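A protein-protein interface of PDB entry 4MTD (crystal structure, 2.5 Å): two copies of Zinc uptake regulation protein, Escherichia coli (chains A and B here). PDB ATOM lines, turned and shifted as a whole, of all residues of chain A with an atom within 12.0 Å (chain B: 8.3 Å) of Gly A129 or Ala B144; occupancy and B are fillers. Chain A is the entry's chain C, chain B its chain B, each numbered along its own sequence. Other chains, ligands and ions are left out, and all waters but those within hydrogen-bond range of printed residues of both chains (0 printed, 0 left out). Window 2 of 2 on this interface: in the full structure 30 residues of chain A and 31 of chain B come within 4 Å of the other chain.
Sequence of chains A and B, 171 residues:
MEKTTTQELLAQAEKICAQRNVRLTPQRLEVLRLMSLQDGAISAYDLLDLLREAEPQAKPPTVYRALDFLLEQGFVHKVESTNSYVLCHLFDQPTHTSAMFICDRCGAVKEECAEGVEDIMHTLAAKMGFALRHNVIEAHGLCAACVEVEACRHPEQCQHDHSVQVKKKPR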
ATOM      1  N   MET A 121      17.926  -0.256   0.323  1.00  0.00           N
ATOM      2  CA  MET A 121      17.097  -1.271  -0.323  1.00  0.00           C
ATOM      3  C   MET A 121      17.883  -1.951  -1.435  1.00  0.00           C
ATOM      4  O   MET A 121      17.909  -3.177  -1.518  1.00  0.00           O
ATOM      5  CB  MET A 121      15.816  -0.641  -0.894  1.00  0.00           C
ATOM      6  CG  MET A 121      14.530  -1.397  -0.582  1.00  0.00           C
ATOM      7  SD  MET A 121      14.159  -1.624   1.170  1.00  0.00           S
ATOM      8  CE  MET A 121      14.397   0.047   1.748  1.00  0.00           C
ATOM      9  N   HIS A 122      18.523  -1.150  -2.283  1.00  0.00           N
ATOM     10  CA  HIS A 122      19.368  -1.677  -3.356  1.00  0.00           C
ATOM     11  C   HIS A 122      20.508  -2.558  -2.833  1.00  0.00           C
ATOM     12  O   HIS A 122      20.883  -3.528  -3.488  1.00  0.00           O
ATOM     13  CB  HIS A 122      19.950  -0.551  -4.204  1.00  0.00           C
ATOM     14  CG  HIS A 122      19.024  -0.046  -5.265  1.00  0.00           C
ATOM     15  ND1 HIS A 122      18.024   0.872  -5.012  1.00  0.00           N
ATOM     16  CD2 HIS A 122      18.963  -0.312  -6.592  1.00  0.00           C
ATOM     17  CE1 HIS A 122      17.385   1.144  -6.136  1.00  0.00           C
ATOM     18  NE2 HIS A 122      17.936   0.441  -7.108  1.00  0.00           N
ATOM     19  N   THR A 123      21.047  -2.234  -1.660  1.00  0.00           N
ATOM     20  CA  THR A 123      22.108  -3.049  -1.073  1.00  0.00           C
ATOM     21  C   THR A 123      21.539  -4.369  -0.568  1.00  0.00           C
ATOM     22  O   THR A 123      22.133  -5.419  -0.790  1.00  0.00           O
ATOM     23  CB  THR A 123      22.885  -2.323   0.058  1.00  0.00           C
ATOM     24  OG1 THR A 123      21.993  -1.968   1.121  1.00  0.00           O
ATOM     25  CG2 THR A 123      23.566  -1.066  -0.462  1.00  0.00           C
ATOM     26  N   LEU A 124      20.387  -4.323   0.100  1.00  0.00           N
ATOM     27  CA  LEU A 124      19.717  -5.558   0.536  1.00  0.00           C
ATOM     28  C   LEU A 124      19.384  -6.468  -0.645  1.00  0.00           C
ATOM     29  O   LEU A 124      19.660  -7.666  -0.609  1.00  0.00           O
ATOM     30  CB  LEU A 124      18.443  -5.252   1.308  1.00  0.00           C
ATOM     31  CG  LEU A 124      18.634  -4.828   2.761  1.00  0.00           C
ATOM     32  CD1 LEU A 124      17.345  -4.204   3.281  1.00  0.00           C
ATOM     33  CD2 LEU A 124      19.061  -6.009   3.623  1.00  0.00           C
ATOM     34  N   ALA A 125      18.804  -5.897  -1.692  1.00  0.00           N
ATOM     35  CA  ALA A 125      18.514  -6.661  -2.900  1.00  0.00           C
ATOM     36  C   ALA A 125      19.786  -7.271  -3.476  1.00  0.00           C
ATOM     37  O   ALA A 125      19.809  -8.454  -3.836  1.00  0.00           O
ATOM     38  CB  ALA A 125      17.842  -5.784  -3.944  1.00  0.00           C
ATOM     39  N   ALA A 126      20.841  -6.461  -3.557  1.00  0.00           N
ATOM     40  CA  ALA A 126      22.106  -6.902  -4.143  1.00  0.00           C
ATOM     41  C   ALA A 126      22.630  -8.186  -3.501  1.00  0.00           C
ATOM     42  O   ALA A 126      23.098  -9.073  -4.204  1.00  0.00           O
ATOM     43  CB  ALA A 126      23.154  -5.800  -4.050  1.00  0.00           C
ATOM     44  N   LYS A 127      22.534  -8.279  -2.177  1.00  0.00           N
ATOM     45  CA  LYS A 127      23.019  -9.442  -1.432  1.00  0.00           C
ATOM     46  C   LYS A 127      22.179 -10.701  -1.670  1.00  0.00           C
ATOM     47  O   LYS A 127      22.709 -11.813  -1.678  1.00  0.00           O
ATOM     48  CB  LYS A 127      23.114  -9.106   0.059  1.00  0.00           C
ATOM     49  CG  LYS A 127      24.205  -8.087   0.323  1.00  0.00           C
ATOM     50  CD  LYS A 127      24.375  -7.710   1.783  1.00  0.00           C
ATOM     51  CE  LYS A 127      25.548  -6.741   1.912  1.00  0.00           C
ATOM     52  NZ  LYS A 127      25.608  -6.061   3.231  1.00  0.00           N
ATOM     53  N   MET A 128      20.877 -10.516  -1.867  1.00  0.00           N
ATOM     54  CA  MET A 128      20.027 -11.552  -2.452  1.00  0.00           C
ATOM     55  C   MET A 128      20.305 -11.511  -3.947  1.00  0.00           C
ATOM     56  O   MET A 128      21.134 -10.739  -4.402  1.00  0.00           O
ATOM     57  CB  MET A 128      18.544 -11.248  -2.214  1.00  0.00           C
ATOM     58  CG  MET A 128      18.148 -10.988  -0.771  1.00  0.00           C
ATOM     59  SD  MET A 128      16.457 -10.355  -0.687  1.00  0.00           S
ATOM     60  CE  MET A 128      16.704  -8.891   0.306  1.00  0.00           C
ATOM     61  N   GLY A 129      19.604 -12.297  -4.740  1.00  0.00           N
ATOM     62  CA  GLY A 129      19.804 -12.193  -6.184  1.00  0.00           C
ATOM     63  C   GLY A 129      18.777 -11.288  -6.819  1.00  0.00           C
ATOM     64  O   GLY A 129      18.395 -11.487  -7.974  1.00  0.00           O
ATOM     65  N   PHE A 130      18.334 -10.277  -6.078  1.00  0.00           N
ATOM     66  CA  PHE A 130      17.083  -9.619  -6.396  1.00  0.00           C
ATOM     67  C   PHE A 130      17.296  -8.467  -7.362  1.00  0.00           C
ATOM     68  O   PHE A 130      18.004  -7.529  -7.046  1.00  0.00           O
ATOM     69  CB  PHE A 130      16.425  -9.145  -5.103  1.00  0.00           C
ATOM     70  CG  PHE A 130      14.946  -8.940  -5.209  1.00  0.00           C
ATOM     71  CD1 PHE A 130      14.064  -9.976  -4.918  1.00  0.00           C
ATOM     72  CD2 PHE A 130      14.431  -7.711  -5.580  1.00  0.00           C
ATOM     73  CE1 PHE A 130      12.695  -9.790  -5.005  1.00  0.00           C
ATOM     74  CE2 PHE A 130      13.058  -7.514  -5.664  1.00  0.00           C
ATOM     75  CZ  PHE A 130      12.195  -8.558  -5.380  1.00  0.00           C
ATOM     76  N   ALA A 131      16.695  -8.558  -8.545  1.00  0.00           N
ATOM     77  CA  ALA A 131      16.662  -7.445  -9.485  1.00  0.00           C
ATOM     78  C   ALA A 131      15.575  -6.442  -9.076  1.00  0.00           C
ATOM     79  O   ALA A 131      14.396  -6.655  -9.371  1.00  0.00           O
ATOM     80  CB  ALA A 131      16.398  -7.954 -10.890  1.00  0.00           C
ATOM     81  N   LEU A 132      15.973  -5.356  -8.410  1.00  0.00           N
ATOM     82  CA  LEU A 132      15.023  -4.389  -7.840  1.00  0.00           C
ATOM     83  C   LEU A 132      14.533  -3.395  -8.881  1.00  0.00           C
ATOM     84  O   LEU A 132      15.306  -2.601  -9.382  1.00  0.00           O
ATOM     85  CB  LEU A 132      15.674  -3.656  -6.665  1.00  0.00           C
ATOM     86  CG  LEU A 132      14.863  -2.690  -5.788  1.00  0.00           C
ATOM     87  CD1 LEU A 132      13.381  -3.005  -5.749  1.00  0.00           C
ATOM     88  CD2 LEU A 132      15.417  -2.691  -4.370  1.00  0.00           C
ATOM     89  N   ARG A 133      13.242  -3.440  -9.198  1.00  0.00           N
ATOM     90  CA  ARG A 133      12.671  -2.601 -10.254  1.00  0.00           C
ATOM     91  C   ARG A 133      12.057  -1.298  -9.718  1.00  0.00           C
ATOM     92  O   ARG A 133      12.170  -0.250 -10.352  1.00  0.00           O
ATOM     93  CB  ARG A 133      11.634  -3.397 -11.051  1.00  0.00           C
ATOM     94  CG  ARG A 133      12.225  -4.626 -11.744  1.00  0.00           C
ATOM     95  CD  ARG A 133      11.168  -5.583 -12.287  1.00  0.00           C
ATOM     96  NE  ARG A 133      10.741  -5.263 -13.652  1.00  0.00           N
ATOM     97  CZ  ARG A 133       9.854  -5.972 -14.354  1.00  0.00           C
ATOM     98  NH1 ARG A 133       9.280  -7.057 -13.830  1.00  0.00           N
ATOM     99  NH2 ARG A 133       9.538  -5.592 -15.590  1.00  0.00           N
ATOM    100  N   PHE B 101      10.509  -7.773  -0.054  1.00  0.00           N
ATOM    101  CA  PHE B 101      10.960  -7.933  -1.413  1.00  0.00           C
ATOM    102  C   PHE B 101      10.015  -8.872  -2.132  1.00  0.00           C
ATOM    103  O   PHE B 101       9.883 -10.033  -1.767  1.00  0.00           O
ATOM    104  CB  PHE B 101      12.393  -8.427  -1.411  1.00  0.00           C
ATOM    105  CG  PHE B 101      13.360  -7.396  -0.926  1.00  0.00           C
ATOM    106  CD1 PHE B 101      14.090  -6.633  -1.827  1.00  0.00           C
ATOM    107  CD2 PHE B 101      13.504  -7.157   0.422  1.00  0.00           C
ATOM    108  CE1 PHE B 101      14.976  -5.673  -1.383  1.00  0.00           C
ATOM    109  CE2 PHE B 101      14.384  -6.196   0.879  1.00  0.00           C
ATOM    110  CZ  PHE B 101      15.124  -5.457  -0.025  1.00  0.00           C
ATOM    111  N   CYS B 103       8.544 -10.546  -5.582  1.00  0.00           N
ATOM    112  CA  CYS B 103       8.804 -10.936  -6.969  1.00  0.00           C
ATOM    113  C   CYS B 103       7.503 -10.861  -7.772  1.00  0.00           C
ATOM    114  O   CYS B 103       6.512 -11.465  -7.398  1.00  0.00           O
ATOM    115  CB  CYS B 103       9.421 -12.344  -7.034  1.00  0.00           C
ATOM    116  SG  CYS B 103       9.691 -13.016  -8.701  1.00  0.00           S
ATOM    117  N   CYS B 106       7.031 -14.994  -9.794  1.00  0.00           N
ATOM    118  CA  CYS B 106       6.622 -16.145  -9.004  1.00  0.00           C
ATOM    119  C   CYS B 106       5.776 -15.751  -7.798  1.00  0.00           C
ATOM    120  O   CYS B 106       5.251 -16.622  -7.101  1.00  0.00           O
ATOM    121  CB  CYS B 106       7.846 -16.940  -8.557  1.00  0.00           C
ATOM    122  SG  CYS B 106       8.817 -16.147  -7.263  1.00  0.00           S
ATOM    123  N   GLY B 141      10.403  -6.485  -7.914  1.00  0.00           N
ATOM    124  CA  GLY B 141      11.393  -6.900  -8.899  1.00  0.00           C
ATOM    125  C   GLY B 141      11.251  -8.345  -9.318  1.00  0.00           C
ATOM    126  O   GLY B 141      10.135  -8.851  -9.430  1.00  0.00           O
ATOM    127  N   LEU B 142      12.387  -8.992  -9.576  1.00  0.00           N
ATOM    128  CA  LEU B 142      12.447 -10.437  -9.774  1.00  0.00           C
ATOM    129  C   LEU B 142      13.347 -11.014  -8.704  1.00  0.00           C
ATOM    130  O   LEU B 142      14.381 -10.423  -8.386  1.00  0.00           O
ATOM    131  CB  LEU B 142      13.007 -10.782 -11.151  1.00  0.00           C
ATOM    132  CG  LEU B 142      12.330 -10.133 -12.358  1.00  0.00           C
ATOM    133  CD1 LEU B 142      13.095 -10.432 -13.639  1.00  0.00           C
ATOM    134  CD2 LEU B 142      10.890 -10.607 -12.475  1.00  0.00           C
ATOM    135  N   CYS B 143      12.957 -12.151  -8.130  1.00  0.00           N
ATOM    136  CA  CYS B 143      13.801 -12.816  -7.141  1.00  0.00           C
ATOM    137  C   CYS B 143      14.952 -13.563  -7.846  1.00  0.00           C
ATOM    138  O   CYS B 143      15.009 -13.614  -9.078  1.00  0.00           O
ATOM    139  CB  CYS B 143      12.968 -13.723  -6.211  1.00  0.00           C
ATOM    140  SG  CYS B 143      12.417 -15.342  -6.833  1.00  0.00           S
ATOM    141  N   ALA B 144      15.880 -14.103  -7.061  1.00  0.00           N
ATOM    142  CA  ALA B 144      17.033 -14.831  -7.610  1.00  0.00           C
ATOM    143  C   ALA B 144      16.579 -15.924  -8.579  1.00  0.00           C
ATOM    144  O   ALA B 144      16.987 -15.947  -9.743  1.00  0.00           O
ATOM    145  CB  ALA B 144      17.875 -15.430  -6.489  1.00  0.00           C
ATOM    146  N   ALA B 145      15.716 -16.811  -8.089  1.00  0.00           N
ATOM    147  CA  ALA B 145      15.147 -17.884  -8.907  1.00  0.00           C
ATOM    148  C   ALA B 145      14.631 -17.395 -10.264  1.00  0.00           C
ATOM    149  O   ALA B 145      15.020 -17.925 -11.307  1.00  0.00           O
ATOM    150  CB  ALA B 145      14.039 -18.595  -8.149  1.00  0.00           C
ATOM    151  N   CYS B 146      13.763 -16.387 -10.254  1.00  0.00           N
ATOM    152  CA  CYS B 146      13.208 -15.859 -11.502  1.00  0.00           C
ATOM    153  C   CYS B 146      14.277 -15.276 -12.432  1.00  0.00           C
ATOM    154  O   CYS B 146      14.075 -15.235 -13.648  1.00  0.00           O
ATOM    155  CB  CYS B 146      12.142 -14.785 -11.240  1.00  0.00           C
ATOM    156  SG  CYS B 146      10.557 -15.390 -10.616  1.00  0.00           S
ATOM    157  N   VAL B 147      15.391 -14.806 -11.867  1.00  0.00           N
ATOM    158  CA  VAL B 147      16.490 -14.275 -12.674  1.00  0.00           C
ATOM    159  C   VAL B 147      17.179 -15.401 -13.463  1.00  0.00           C
ATOM    160  O   VAL B 147      17.374 -15.275 -14.675  1.00  0.00           O
ATOM    161  CB  VAL B 147      17.511 -13.482 -11.818  1.00  0.00           C
ATOM    162  CG1 VAL B 147      18.730 -13.077 -12.640  1.00  0.00           C
ATOM    163  CG2 VAL B 147      16.857 -12.246 -11.217  1.00  0.00           C
ATOM    164  N   GLU B 148      17.534 -16.492 -12.779  1.00  0.00           N
ATOM    165  CA  GLU B 148      18.108 -17.671 -13.442  1.00  0.00           C
ATOM    166  C   GLU B 148      17.267 -18.073 -14.638  1.00  0.00           C
ATOM    167  O   GLU B 148      17.765 -18.145 -15.758  1.00  0.00           O
ATOM    168  CB  GLU B 148      18.184 -18.861 -12.486  1.00  0.00           C
ATOM    169  CG  GLU B 148      19.318 -18.800 -11.483  1.00  0.00           C
ATOM    170  CD  GLU B 148      19.433 -20.078 -10.673  1.00  0.00           C
ATOM    171  OE1 GLU B 148      18.407 -20.523 -10.106  1.00  0.00           O
ATOM    172  OE2 GLU B 148      20.548 -20.640 -10.605  1.00  0.00           O
ATOM    173  N   VAL B 149      15.985 -18.318 -14.381  1.00  0.00           N
ATOM    174  CA  VAL B 149      15.035 -18.726 -15.413  1.00  0.00           C
ATOM    175  C   VAL B 149      14.998 -17.730 -16.568  1.00  0.00           C
ATOM    176  O   VAL B 149      15.058 -18.124 -17.732  1.00  0.00           O
ATOM    177  CB  VAL B 149      13.613 -18.889 -14.827  1.00  0.00           C
ATOM    178  CG1 VAL B 149      12.562 -18.973 -15.931  1.00  0.00           C
ATOM    179  CG2 VAL B 149      13.553 -20.114 -13.922  1.00  0.00           C
ATOM    180  N   GLU B 150      14.908 -16.444 -16.243  1.00  0.00           N
ATOM    181  CA  GLU B 150      14.803 -15.396 -17.263  1.00  0.00           C
ATOM    182  C   GLU B 150      16.070 -15.292 -18.125  1.00  0.00           C
ATOM    183  O   GLU B 150      16.000 -14.890 -19.287  1.00  0.00           O
ATOM    184  CB  GLU B 150      14.485 -14.046 -16.606  1.00  0.00           C
ATOM    185  CG  GLU B 150      13.915 -12.996 -17.549  1.00  0.00           C
ATOM    186  CD  GLU B 150      12.459 -13.253 -17.880  1.00  0.00           C
ATOM    187  OE1 GLU B 150      11.585 -12.858 -17.079  1.00  0.00           O
ATOM    188  OE2 GLU B 150      12.189 -13.852 -18.939  1.00  0.00           O
ATOM    189  N   ALA B 151      17.221 -15.661 -17.559  1.00  0.00           N
ATOM    190  CA  ALA B 151      18.485 -15.693 -18.309  1.00  0.00           C
ATOM    191  C   ALA B 151      18.473 -16.715 -19.460  1.00  0.00           C
ATOM    192  O   ALA B 151      19.147 -16.516 -20.471  1.00  0.00           O
ATOM    193  CB  ALA B 151      19.652 -15.967 -17.368  1.00  0.00           C
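The backbone carbonyl oxygen (O) of Ala A125 lies within hydrogen-bond range of the backbone NH (N) of Phe A130.
Of chain B, only Ala B144 and Val B147 come within 4 Å of Gly A129. Of chain A, only Phe A130 comes within 4 Å of Cys B143. No residue of chain A comes within 4 Å of Cys B146. Of chain A, only Gly A129 comes within 4 Å of Val B147. Printed residues of chain B within 4 Å of Leu A124: Phe B101 (3.6 Å). Of the printed residues of chain A, Gly B141 touches Phe A130 (3.6 Å), Ala A131 (3.0 Å) and Arg A133 (3.6 Å). Printed residues of chain B within 4 Å of Ala A131: Gly B141 and Leu B142. Ala B151 touches none of the printed residues of chain A. Cys B103 touches none of the printed residues of chain A. The nearest printed residue of chain B that does not touch Phe A130 is Cys B103 (4.2 Å).
No position is printed for both chains.
Among the printed residues, pairs that only touch across the chains: Ala A131 with Gly B141 (3.0 Å), Phe A130 with Leu B142 (3.5 Å), Leu A124 with Phe B101 (3.6 Å), Met A128 with Phe B101 (3.6 Å), Phe A130 with Cys B143 (3.6 Å), Gly A129 with Ala B144 (3.6 Å), Phe A130 with Gly B141 (3.6 Å), Arg A133 with Gly B141 (3.6 Å), Gly A129 with Val B147 (3.7 Å), Ala A125 with Phe B101 (3.8 Å), Met A121 with Phe B101 (3.9 Å) and Phe A130 with Phe B101 (3.9 Å).
Of the 13 printed residues of chain A, 8 touch a printed residue of chain B. Printed residues of chain A that touch a printed residue of chain B: Met A121, Leu A124, Ala A125, Met A128, Gly A129, Phe A130, Ala A131 and Arg A133. Of the 14 printed residues of chain B, 6 touch a printed residue of chain A. Hydrophobic or aromatic side chains of chain B that line the printed part of chain A: Phe B101, Ala B144 and Val B147. Along chain B the printed residues that touch a printed residue of chain A span positions 101 to 147. Among the printed residues, 13 pairs touch across the chains.
The backbone carbonyl oxygen (O) of Leu B142 lies within hydrogen-bond range of the backbone NH (N) of Ala A131 (3.0 Å).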
